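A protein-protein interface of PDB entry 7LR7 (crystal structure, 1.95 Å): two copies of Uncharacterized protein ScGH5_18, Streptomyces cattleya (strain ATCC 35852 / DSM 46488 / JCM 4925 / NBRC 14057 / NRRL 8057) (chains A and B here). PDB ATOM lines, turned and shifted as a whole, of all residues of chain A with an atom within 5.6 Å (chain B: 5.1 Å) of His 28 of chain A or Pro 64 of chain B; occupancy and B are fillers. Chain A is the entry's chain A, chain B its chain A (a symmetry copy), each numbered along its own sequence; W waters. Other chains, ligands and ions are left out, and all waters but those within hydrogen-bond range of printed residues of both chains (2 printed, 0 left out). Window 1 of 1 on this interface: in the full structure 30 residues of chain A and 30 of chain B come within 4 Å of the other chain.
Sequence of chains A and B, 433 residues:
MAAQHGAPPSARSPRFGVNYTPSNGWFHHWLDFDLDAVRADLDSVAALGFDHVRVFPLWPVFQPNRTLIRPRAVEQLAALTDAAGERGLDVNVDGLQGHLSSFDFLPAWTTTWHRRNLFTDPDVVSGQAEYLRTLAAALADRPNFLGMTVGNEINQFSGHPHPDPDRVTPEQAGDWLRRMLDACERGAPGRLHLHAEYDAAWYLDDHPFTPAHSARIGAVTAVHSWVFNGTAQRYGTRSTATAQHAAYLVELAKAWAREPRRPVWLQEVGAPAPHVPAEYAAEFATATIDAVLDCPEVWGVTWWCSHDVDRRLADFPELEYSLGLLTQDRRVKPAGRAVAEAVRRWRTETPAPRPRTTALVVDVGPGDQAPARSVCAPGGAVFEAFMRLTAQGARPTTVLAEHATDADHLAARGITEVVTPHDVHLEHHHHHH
No position is printed for both chains.
Of the 9 pairs that touch across the chains among the printed residues, none has its exchanged pair printed and touching as well.
Water W2 bridges O of Leu 31 of chain A (2.4 Å) and NH2 of Arg 70 of chain B (3.4 Å).
Water W1 lies within hydrogen-bond range of a ring nitrogen (NE2) of His 28 of chain A (2.8 Å) and the side-chain amide nitrogen (ND2) of Asn 65 of chain B (2.9 Å).
The guanidinium group (NH2) of Arg 70 of chain B is in hydrogen-bond range of the backbone carbonyl oxygen (O) of Leu 31 of chain A (3.2 Å).
The guanidinium group (NE) of Arg 70 of chain B lies within salt-bridge range of the side-chain carboxylate (OD2) of Asp 32 of chain A (2.6 Å).
Of the 11 printed residues of chain A, 5 touch a printed residue of chain B.
Hydrophobic or aromatic side chains of chain A that line the printed part of chain B: His 28, Leu 31, Phe 105 and Leu 313.
Among the printed residues, 9 pairs touch across the chains.
Among the printed residues, Asp or Glu carboxylates within 4 Å of a Lys or Arg side-chain nitrogen of the other chain: Asp 32 of chain A with Arg 70 of chain B (2.6 Å).
ND1 of His 28 of chain A touches CB of Pro 64 of chain B, at 3.5 Å.
His 28 of chain A touches Asn 65 of chain B.
O of Val 61 of chain B touches CD1 of Leu 31 of chain A (3.8 Å).
Leu 31 of chain A touches Pro 64 of chain B.
Phe 105 of chain A touches Ala 108 of chain B.
OD1 of Asn 65 of chain B touches CA of Leu 313 of chain A (3.7 Å).
Leu 68 of chain B touches Leu 313 of chain A.
Of chain B, only Pro 64 and Asn 65 come within 4 Å of His 28 of chain A.
Pro 64 of chain B touches just these residues of chain A: His 28 and Leu 31.
Of the printed residues of chain B, Leu 31 of chain A touches Val 61 (3.8 Å), Pro 64 (3.8 Å) and Arg 70 (3.2 Å).
Of the printed residues of chain A, Asn 65 of chain B touches His 28 (3.96 Å) and Leu 313 (3.7 Å).
Of the printed residues of chain A, Val 61 of chain B touches Leu 31 (3.8 Å).
Trp 109 of chain B touches none of the printed residues of chain A.
Gly 25 of chain A touches none of the printed residues of chain B.
The nearest residue of chain B that does not touch His 28 of chain A is Leu 68 of chain B (4.3 Å).
The nearest printed residue of chain A that does not touch Val 61 of chain B is Asp 32 of chain A (6.6 Å).
The guanidinium group (NH1) of Arg 70 of chain B is in hydrogen-bond range of the backbone carbonyl oxygen (O) of Val 61 of chain B, 3.0 Å away.
N of Arg 70 of chain B is in hydrogen-bond range of O of Phe 62 of chain B.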
ATOM      1  N   GLY A  25      -1.390  30.308  17.425  1.00  0.00           N
ATOM      2  CA  GLY A  25      -0.137  29.697  17.053  1.00  0.00           C
ATOM      3  C   GLY A  25       1.003  29.890  18.029  1.00  0.00           C
ATOM      4  O   GLY A  25       2.109  29.411  17.750  1.00  0.00           O
ATOM      5  N   TRP A  26       0.776  30.555  19.158  1.00  0.00           N
ATOM      6  CA  TRP A  26       1.811  30.727  20.197  1.00  0.00           C
ATOM      7  C   TRP A  26       3.022  31.428  19.559  1.00  0.00           C
ATOM      8  O   TRP A  26       2.875  32.230  18.629  1.00  0.00           O
ATOM      9  CB  TRP A  26       2.091  29.375  20.842  1.00  0.00           C
ATOM     10  CG  TRP A  26       2.961  29.340  22.109  1.00  0.00           C
ATOM     11  CD1 TRP A  26       2.665  29.863  23.341  1.00  0.00           C
ATOM     12  CD2 TRP A  26       4.242  28.689  22.250  1.00  0.00           C
ATOM     13  NE1 TRP A  26       3.694  29.609  24.230  1.00  0.00           N
ATOM     14  CE2 TRP A  26       4.662  28.876  23.589  1.00  0.00           C
ATOM     15  CE3 TRP A  26       5.080  27.987  21.365  1.00  0.00           C
ATOM     16  CZ2 TRP A  26       5.887  28.383  24.066  1.00  0.00           C
ATOM     17  CZ3 TRP A  26       6.288  27.476  21.848  1.00  0.00           C
ATOM     18  CH2 TRP A  26       6.681  27.687  23.184  1.00  0.00           C
ATOM     19  N   PHE A  27       4.232  31.134  20.020  1.00  0.00           N
ATOM     20  CA  PHE A  27       5.399  31.788  19.444  1.00  0.00           C
ATOM     21  C   PHE A  27       5.706  31.319  18.031  1.00  0.00           C
ATOM     22  O   PHE A  27       6.514  31.958  17.348  1.00  0.00           O
ATOM     23  CB  PHE A  27       6.592  31.589  20.375  1.00  0.00           C
ATOM     24  CG  PHE A  27       6.379  32.239  21.717  1.00  0.00           C
ATOM     25  CD1 PHE A  27       6.082  33.598  21.788  1.00  0.00           C
ATOM     26  CD2 PHE A  27       6.405  31.495  22.883  1.00  0.00           C
ATOM     27  CE1 PHE A  27       5.861  34.205  22.989  1.00  0.00           C
ATOM     28  CE2 PHE A  27       6.181  32.096  24.104  1.00  0.00           C
ATOM     29  CZ  PHE A  27       5.898  33.454  24.155  1.00  0.00           C
ATOM     30  N   HIS A  28       5.055  30.249  17.573  1.00  0.00           N
ATOM     31  CA  HIS A  28       5.121  29.829  16.180  1.00  0.00           C
ATOM     32  C   HIS A  28       4.384  30.772  15.241  1.00  0.00           C
ATOM     33  O   HIS A  28       4.505  30.613  14.021  1.00  0.00           O
ATOM     34  CB  HIS A  28       4.564  28.410  16.029  1.00  0.00           C
ATOM     35  CG  HIS A  28       5.180  27.420  16.970  1.00  0.00           C
ATOM     36  ND1 HIS A  28       6.537  27.164  16.999  1.00  0.00           N
ATOM     37  CD2 HIS A  28       4.631  26.639  17.930  1.00  0.00           C
ATOM     38  CE1 HIS A  28       6.790  26.255  17.924  1.00  0.00           C
ATOM     39  NE2 HIS A  28       5.651  25.924  18.505  1.00  0.00           N
ATOM     40  N   HIS A  29       3.647  31.760  15.768  1.00  0.00           N
ATOM     41  CA  HIS A  29       2.957  32.688  14.885  1.00  0.00           C
ATOM     42  C   HIS A  29       3.910  33.444  13.955  1.00  0.00           C
ATOM     43  O   HIS A  29       3.445  34.012  12.961  1.00  0.00           O
ATOM     44  CB  HIS A  29       2.139  33.684  15.702  1.00  0.00           C
ATOM     45  CG  HIS A  29       2.957  34.809  16.260  1.00  0.00           C
ATOM     46  ND1 HIS A  29       2.643  36.136  16.045  1.00  0.00           N
ATOM     47  CD2 HIS A  29       4.078  34.804  17.017  1.00  0.00           C
ATOM     48  CE1 HIS A  29       3.541  36.898  16.644  1.00  0.00           C
ATOM     49  NE2 HIS A  29       4.425  36.115  17.236  1.00  0.00           N
ATOM     50  N   TRP A  30       5.220  33.484  14.242  1.00  0.00           N
ATOM     51  CA  TRP A  30       6.117  34.161  13.306  1.00  0.00           C
ATOM     52  C   TRP A  30       6.126  33.453  11.963  1.00  0.00           C
ATOM     53  O   TRP A  30       6.386  34.085  10.935  1.00  0.00           O
ATOM     54  CB  TRP A  30       7.551  34.252  13.853  1.00  0.00           C
ATOM     55  CG  TRP A  30       7.705  35.028  15.134  1.00  0.00           C
ATOM     56  CD1 TRP A  30       7.950  34.511  16.374  1.00  0.00           C
ATOM     57  CD2 TRP A  30       7.617  36.450  15.298  1.00  0.00           C
ATOM     58  NE1 TRP A  30       8.016  35.518  17.293  1.00  0.00           N
ATOM     59  CE2 TRP A  30       7.816  36.721  16.662  1.00  0.00           C
ATOM     60  CE3 TRP A  30       7.377  37.516  14.422  1.00  0.00           C
ATOM     61  CZ2 TRP A  30       7.796  38.022  17.185  1.00  0.00           C
ATOM     62  CZ3 TRP A  30       7.346  38.821  14.940  1.00  0.00           C
ATOM     63  CH2 TRP A  30       7.566  39.056  16.311  1.00  0.00           C
ATOM     64  N   LEU A  31       5.846  32.144  11.949  1.00  0.00           N
ATOM     65  CA  LEU A  31       5.813  31.400  10.693  1.00  0.00           C
ATOM     66  C   LEU A  31       4.599  31.751   9.845  1.00  0.00           C
ATOM     67  O   LEU A  31       4.616  31.512   8.634  1.00  0.00           O
ATOM     68  CB  LEU A  31       5.817  29.900  10.968  1.00  0.00           C
ATOM     69  CG  LEU A  31       7.022  29.388  11.753  1.00  0.00           C
ATOM     70  CD1 LEU A  31       6.827  27.900  12.085  1.00  0.00           C
ATOM     71  CD2 LEU A  31       8.291  29.598  10.949  1.00  0.00           C
ATOM     72  N   ASP A  32       3.543  32.287  10.459  1.00  0.00           N
ATOM     73  CA  ASP A  32       2.310  32.651   9.774  1.00  0.00           C
ATOM     74  C   ASP A  32       1.852  34.009  10.308  1.00  0.00           C
ATOM     75  O   ASP A  32       0.755  34.161  10.831  1.00  0.00           O
ATOM     76  CB  ASP A  32       1.206  31.609   9.992  1.00  0.00           C
ATOM     77  CG  ASP A  32       1.565  30.231   9.455  1.00  0.00           C
ATOM     78  OD1 ASP A  32       1.620  30.061   8.223  1.00  0.00           O
ATOM     79  OD2 ASP A  32       1.768  29.308  10.274  1.00  0.00           O
ATOM     80  N   LEU A  58      11.452  34.100  17.784  1.00  0.00           N
ATOM     81  CA  LEU A  58      12.088  32.792  17.804  1.00  0.00           C
ATOM     82  C   LEU A  58      13.412  32.932  17.062  1.00  0.00           C
ATOM     83  O   LEU A  58      13.428  33.142  15.845  1.00  0.00           O
ATOM     84  CB  LEU A  58      11.190  31.730  17.183  1.00  0.00           C
ATOM     85  CG  LEU A  58      10.001  31.296  18.058  1.00  0.00           C
ATOM     86  CD1 LEU A  58       9.330  30.031  17.497  1.00  0.00           C
ATOM     87  CD2 LEU A  58      10.438  31.070  19.504  1.00  0.00           C
ATOM     88  N   PHE A 105      14.692  26.220  21.334  1.00  0.00           N
ATOM     89  CA  PHE A 105      14.739  26.553  19.908  1.00  0.00           C
ATOM     90  C   PHE A 105      16.165  26.962  19.548  1.00  0.00           C
ATOM     91  O   PHE A 105      16.588  28.092  19.804  1.00  0.00           O
ATOM     92  CB  PHE A 105      13.731  27.646  19.580  1.00  0.00           C
ATOM     93  CG  PHE A 105      12.319  27.252  19.873  1.00  0.00           C
ATOM     94  CD1 PHE A 105      11.725  27.604  21.073  1.00  0.00           C
ATOM     95  CD2 PHE A 105      11.590  26.514  18.960  1.00  0.00           C
ATOM     96  CE1 PHE A 105      10.426  27.224  21.359  1.00  0.00           C
ATOM     97  CE2 PHE A 105      10.293  26.137  19.235  1.00  0.00           C
ATOM     98  CZ  PHE A 105       9.709  26.491  20.443  1.00  0.00           C
ATOM     99  N   LEU A 313      -1.889  22.297  21.006  1.00  0.00           N
ATOM    100  CA  LEU A 313      -0.452  22.194  20.873  1.00  0.00           C
ATOM    101  C   LEU A 313       0.029  21.186  21.896  1.00  0.00           C
ATOM    102  O   LEU A 313      -0.441  21.178  23.042  1.00  0.00           O
ATOM    103  CB  LEU A 313       0.219  23.562  21.082  1.00  0.00           C
ATOM    104  CG  LEU A 313      -0.065  24.617  20.016  1.00  0.00           C
ATOM    105  CD1 LEU A 313       0.493  26.024  20.426  1.00  0.00           C
ATOM    106  CD2 LEU A 313       0.510  24.197  18.657  1.00  0.00           C
ATOM    107  N   TRP B  59      11.308  20.127   7.746  1.00  0.00           N
ATOM    108  CA  TRP B  59      10.420  19.495   8.724  1.00  0.00           C
ATOM    109  C   TRP B  59      10.018  20.399   9.886  1.00  0.00           C
ATOM    110  O   TRP B  59       8.805  20.565  10.108  1.00  0.00           O
ATOM    111  CB  TRP B  59      11.073  18.195   9.204  1.00  0.00           C
ATOM    112  CG  TRP B  59      10.244  17.390  10.195  1.00  0.00           C
ATOM    113  CD1 TRP B  59       8.871  17.396  10.344  1.00  0.00           C
ATOM    114  CD2 TRP B  59      10.746  16.475  11.163  1.00  0.00           C
ATOM    115  NE1 TRP B  59       8.506  16.534  11.349  1.00  0.00           N
ATOM    116  CE2 TRP B  59       9.639  15.952  11.866  1.00  0.00           C
ATOM    117  CE3 TRP B  59      12.034  16.032  11.501  1.00  0.00           C
ATOM    118  CZ2 TRP B  59       9.779  15.009  12.885  1.00  0.00           C
ATOM    119  CZ3 TRP B  59      12.173  15.106  12.514  1.00  0.00           C
ATOM    120  CH2 TRP B  59      11.050  14.601  13.198  1.00  0.00           C
ATOM    121  N   PRO B  60      10.932  21.033  10.633  1.00  0.00           N
ATOM    122  CA  PRO B  60      10.467  21.861  11.768  1.00  0.00           C
ATOM    123  C   PRO B  60       9.747  23.145  11.350  1.00  0.00           C
ATOM    124  O   PRO B  60       8.973  23.686  12.150  1.00  0.00           O
ATOM    125  CB  PRO B  60      11.751  22.148  12.570  1.00  0.00           C
ATOM    126  CG  PRO B  60      12.873  21.806  11.711  1.00  0.00           C
ATOM    127  CD  PRO B  60      12.406  20.961  10.560  1.00  0.00           C
ATOM    128  N   VAL B  61       9.934  23.630  10.121  1.00  0.00           N
ATOM    129  CA  VAL B  61       9.132  24.753   9.640  1.00  0.00           C
ATOM    130  C   VAL B  61       7.712  24.297   9.322  1.00  0.00           C
ATOM    131  O   VAL B  61       6.743  25.033   9.550  1.00  0.00           O
ATOM    132  CB  VAL B  61       9.810  25.395   8.413  1.00  0.00           C
ATOM    133  CG1 VAL B  61       8.914  26.437   7.780  1.00  0.00           C
ATOM    134  CG2 VAL B  61      11.174  26.003   8.817  1.00  0.00           C
ATOM    135  N   PHE B  62       7.562  23.083   8.789  1.00  0.00           N
ATOM    136  CA  PHE B  62       6.230  22.560   8.487  1.00  0.00           C
ATOM    137  C   PHE B  62       5.522  22.032   9.726  1.00  0.00           C
ATOM    138  O   PHE B  62       4.295  22.136   9.818  1.00  0.00           O
ATOM    139  CB  PHE B  62       6.312  21.452   7.426  1.00  0.00           C
ATOM    140  CG  PHE B  62       6.497  21.980   6.017  1.00  0.00           C
ATOM    141  CD1 PHE B  62       7.543  22.849   5.719  1.00  0.00           C
ATOM    142  CD2 PHE B  62       5.618  21.629   5.004  1.00  0.00           C
ATOM    143  CE1 PHE B  62       7.714  23.352   4.443  1.00  0.00           C
ATOM    144  CE2 PHE B  62       5.790  22.125   3.705  1.00  0.00           C
ATOM    145  CZ  PHE B  62       6.833  22.986   3.433  1.00  0.00           C
ATOM    146  N   GLN B  63       6.260  21.465  10.674  1.00  0.00           N
ATOM    147  CA  GLN B  63       5.690  20.877  11.888  1.00  0.00           C
ATOM    148  C   GLN B  63       6.400  21.444  13.115  1.00  0.00           C
ATOM    149  O   GLN B  63       7.088  20.718  13.844  1.00  0.00           O
ATOM    150  CB  GLN B  63       5.797  19.350  11.853  1.00  0.00           C
ATOM    151  CG  GLN B  63       4.914  18.593  12.879  1.00  0.00           C
ATOM    152  CD  GLN B  63       4.911  17.078  12.623  1.00  0.00           C
ATOM    153  OE1 GLN B  63       5.793  16.552  11.931  1.00  0.00           O
ATOM    154  NE2 GLN B  63       3.914  16.382  13.157  1.00  0.00           N
ATOM    155  N   PRO B  64       6.229  22.740  13.392  1.00  0.00           N
ATOM    156  CA  PRO B  64       6.978  23.346  14.509  1.00  0.00           C
ATOM    157  C   PRO B  64       6.570  22.803  15.878  1.00  0.00           C
ATOM    158  O   PRO B  64       7.324  22.960  16.843  1.00  0.00           O
ATOM    159  CB  PRO B  64       6.663  24.844  14.372  1.00  0.00           C
ATOM    160  CG  PRO B  64       5.279  24.853  13.724  1.00  0.00           C
ATOM    161  CD  PRO B  64       5.314  23.702  12.747  1.00  0.00           C
ATOM    162  N   ASN B  65       5.415  22.152  15.978  1.00  0.00           N
ATOM    163  CA  ASN B  65       4.974  21.497  17.198  1.00  0.00           C
ATOM    164  C   ASN B  65       4.351  20.169  16.783  1.00  0.00           C
ATOM    165  O   ASN B  65       3.751  20.080  15.714  1.00  0.00           O
ATOM    166  CB  ASN B  65       3.975  22.381  17.967  1.00  0.00           C
ATOM    167  CG  ASN B  65       3.358  21.670  19.155  1.00  0.00           C
ATOM    168  OD1 ASN B  65       2.454  20.846  18.995  1.00  0.00           O
ATOM    169  ND2 ASN B  65       3.843  21.989  20.358  1.00  0.00           N
ATOM    170  N   ARG B  66       4.499  19.142  17.625  1.00  0.00           N
ATOM    171  CA  ARG B  66       4.088  17.794  17.223  1.00  0.00           C
ATOM    172  C   ARG B  66       2.693  17.765  16.595  1.00  0.00           C
ATOM    173  O   ARG B  66       2.465  17.063  15.602  1.00  0.00           O
ATOM    174  CB  ARG B  66       4.133  16.842  18.413  1.00  0.00           C
ATOM    175  CG  ARG B  66       3.757  15.419  18.013  1.00  0.00           C
ATOM    176  CD  ARG B  66       4.398  14.416  18.937  1.00  0.00           C
ATOM    177  NE  ARG B  66       3.972  14.621  20.320  1.00  0.00           N
ATOM    178  CZ  ARG B  66       2.872  14.082  20.846  1.00  0.00           C
ATOM    179  NH1 ARG B  66       2.063  13.309  20.119  1.00  0.00           N
ATOM    180  NH2 ARG B  66       2.578  14.314  22.106  1.00  0.00           N
ATOM    181  N   LEU B  68       1.117  20.553  15.337  1.00  0.00           N
ATOM    182  CA  LEU B  68       0.898  21.684  14.440  1.00  0.00           C
ATOM    183  C   LEU B  68       1.637  21.403  13.138  1.00  0.00           C
ATOM    184  O   LEU B  68       2.847  21.629  13.043  1.00  0.00           O
ATOM    185  CB  LEU B  68       1.354  23.004  15.052  1.00  0.00           C
ATOM    186  CG  LEU B  68       1.288  24.229  14.131  1.00  0.00           C
ATOM    187  CD1 LEU B  68      -0.034  24.367  13.418  1.00  0.00           C
ATOM    188  CD2 LEU B  68       1.602  25.522  14.923  1.00  0.00           C
ATOM    189  N   ARG B  70       1.541  22.944   9.635  1.00  0.00           N
ATOM    190  CA  ARG B  70       1.047  24.246   9.179  1.00  0.00           C
ATOM    191  C   ARG B  70       0.358  24.149   7.826  1.00  0.00           C
ATOM    192  O   ARG B  70       1.020  23.836   6.824  1.00  0.00           O
ATOM    193  CB  ARG B  70       2.211  25.246   9.098  1.00  0.00           C
ATOM    194  CG  ARG B  70       2.792  25.638  10.461  1.00  0.00           C
ATOM    195  CD  ARG B  70       3.904  26.692  10.319  1.00  0.00           C
ATOM    196  NE  ARG B  70       3.572  27.661   9.277  1.00  0.00           N
ATOM    197  CZ  ARG B  70       4.253  27.833   8.152  1.00  0.00           C
ATOM    198  NH1 ARG B  70       5.344  27.124   7.916  1.00  0.00           N
ATOM    199  NH2 ARG B  70       3.843  28.735   7.266  1.00  0.00           N
ATOM    200  N   ALA B 108      12.015  21.330  17.802  1.00  0.00           N
ATOM    201  CA  ALA B 108      12.250  21.480  19.233  1.00  0.00           C
ATOM    202  C   ALA B 108      11.602  20.357  20.026  1.00  0.00           C
ATOM    203  O   ALA B 108      12.085  20.001  21.107  1.00  0.00           O
ATOM    204  CB  ALA B 108      11.729  22.836  19.713  1.00  0.00           C
ATOM    205  N   TRP B 109      10.520  19.773  19.511  1.00  0.00           N
ATOM    206  CA  TRP B 109       9.856  18.722  20.271  1.00  0.00           C
ATOM    207  C   TRP B 109      10.527  17.352  20.119  1.00  0.00           C
ATOM    208  O   TRP B 109       9.964  16.358  20.596  1.00  0.00           O
ATOM    209  CB  TRP B 109       8.378  18.636  19.883  1.00  0.00           C
ATOM    210  CG  TRP B 109       8.103  18.582  18.415  1.00  0.00           C
ATOM    211  CD1 TRP B 109       7.974  19.644  17.553  1.00  0.00           C
ATOM    212  CD2 TRP B 109       7.887  17.401  17.632  1.00  0.00           C
ATOM    213  NE1 TRP B 109       7.690  19.190  16.281  1.00  0.00           N
ATOM    214  CE2 TRP B 109       7.632  17.818  16.302  1.00  0.00           C
ATOM    215  CE3 TRP B 109       7.882  16.034  17.925  1.00  0.00           C
ATOM    216  CZ2 TRP B 109       7.380  16.908  15.261  1.00  0.00           C
ATOM    217  CZ3 TRP B 109       7.623  15.122  16.878  1.00  0.00           C
ATOM    218  CH2 TRP B 109       7.376  15.573  15.571  1.00  0.00           C
HETATM  219  O   HOH W   1       5.719  24.182  20.695  1.00  0.00           O
HETATM  220  O   HOH W   2       6.559  30.752   7.394  1.00  0.00           O
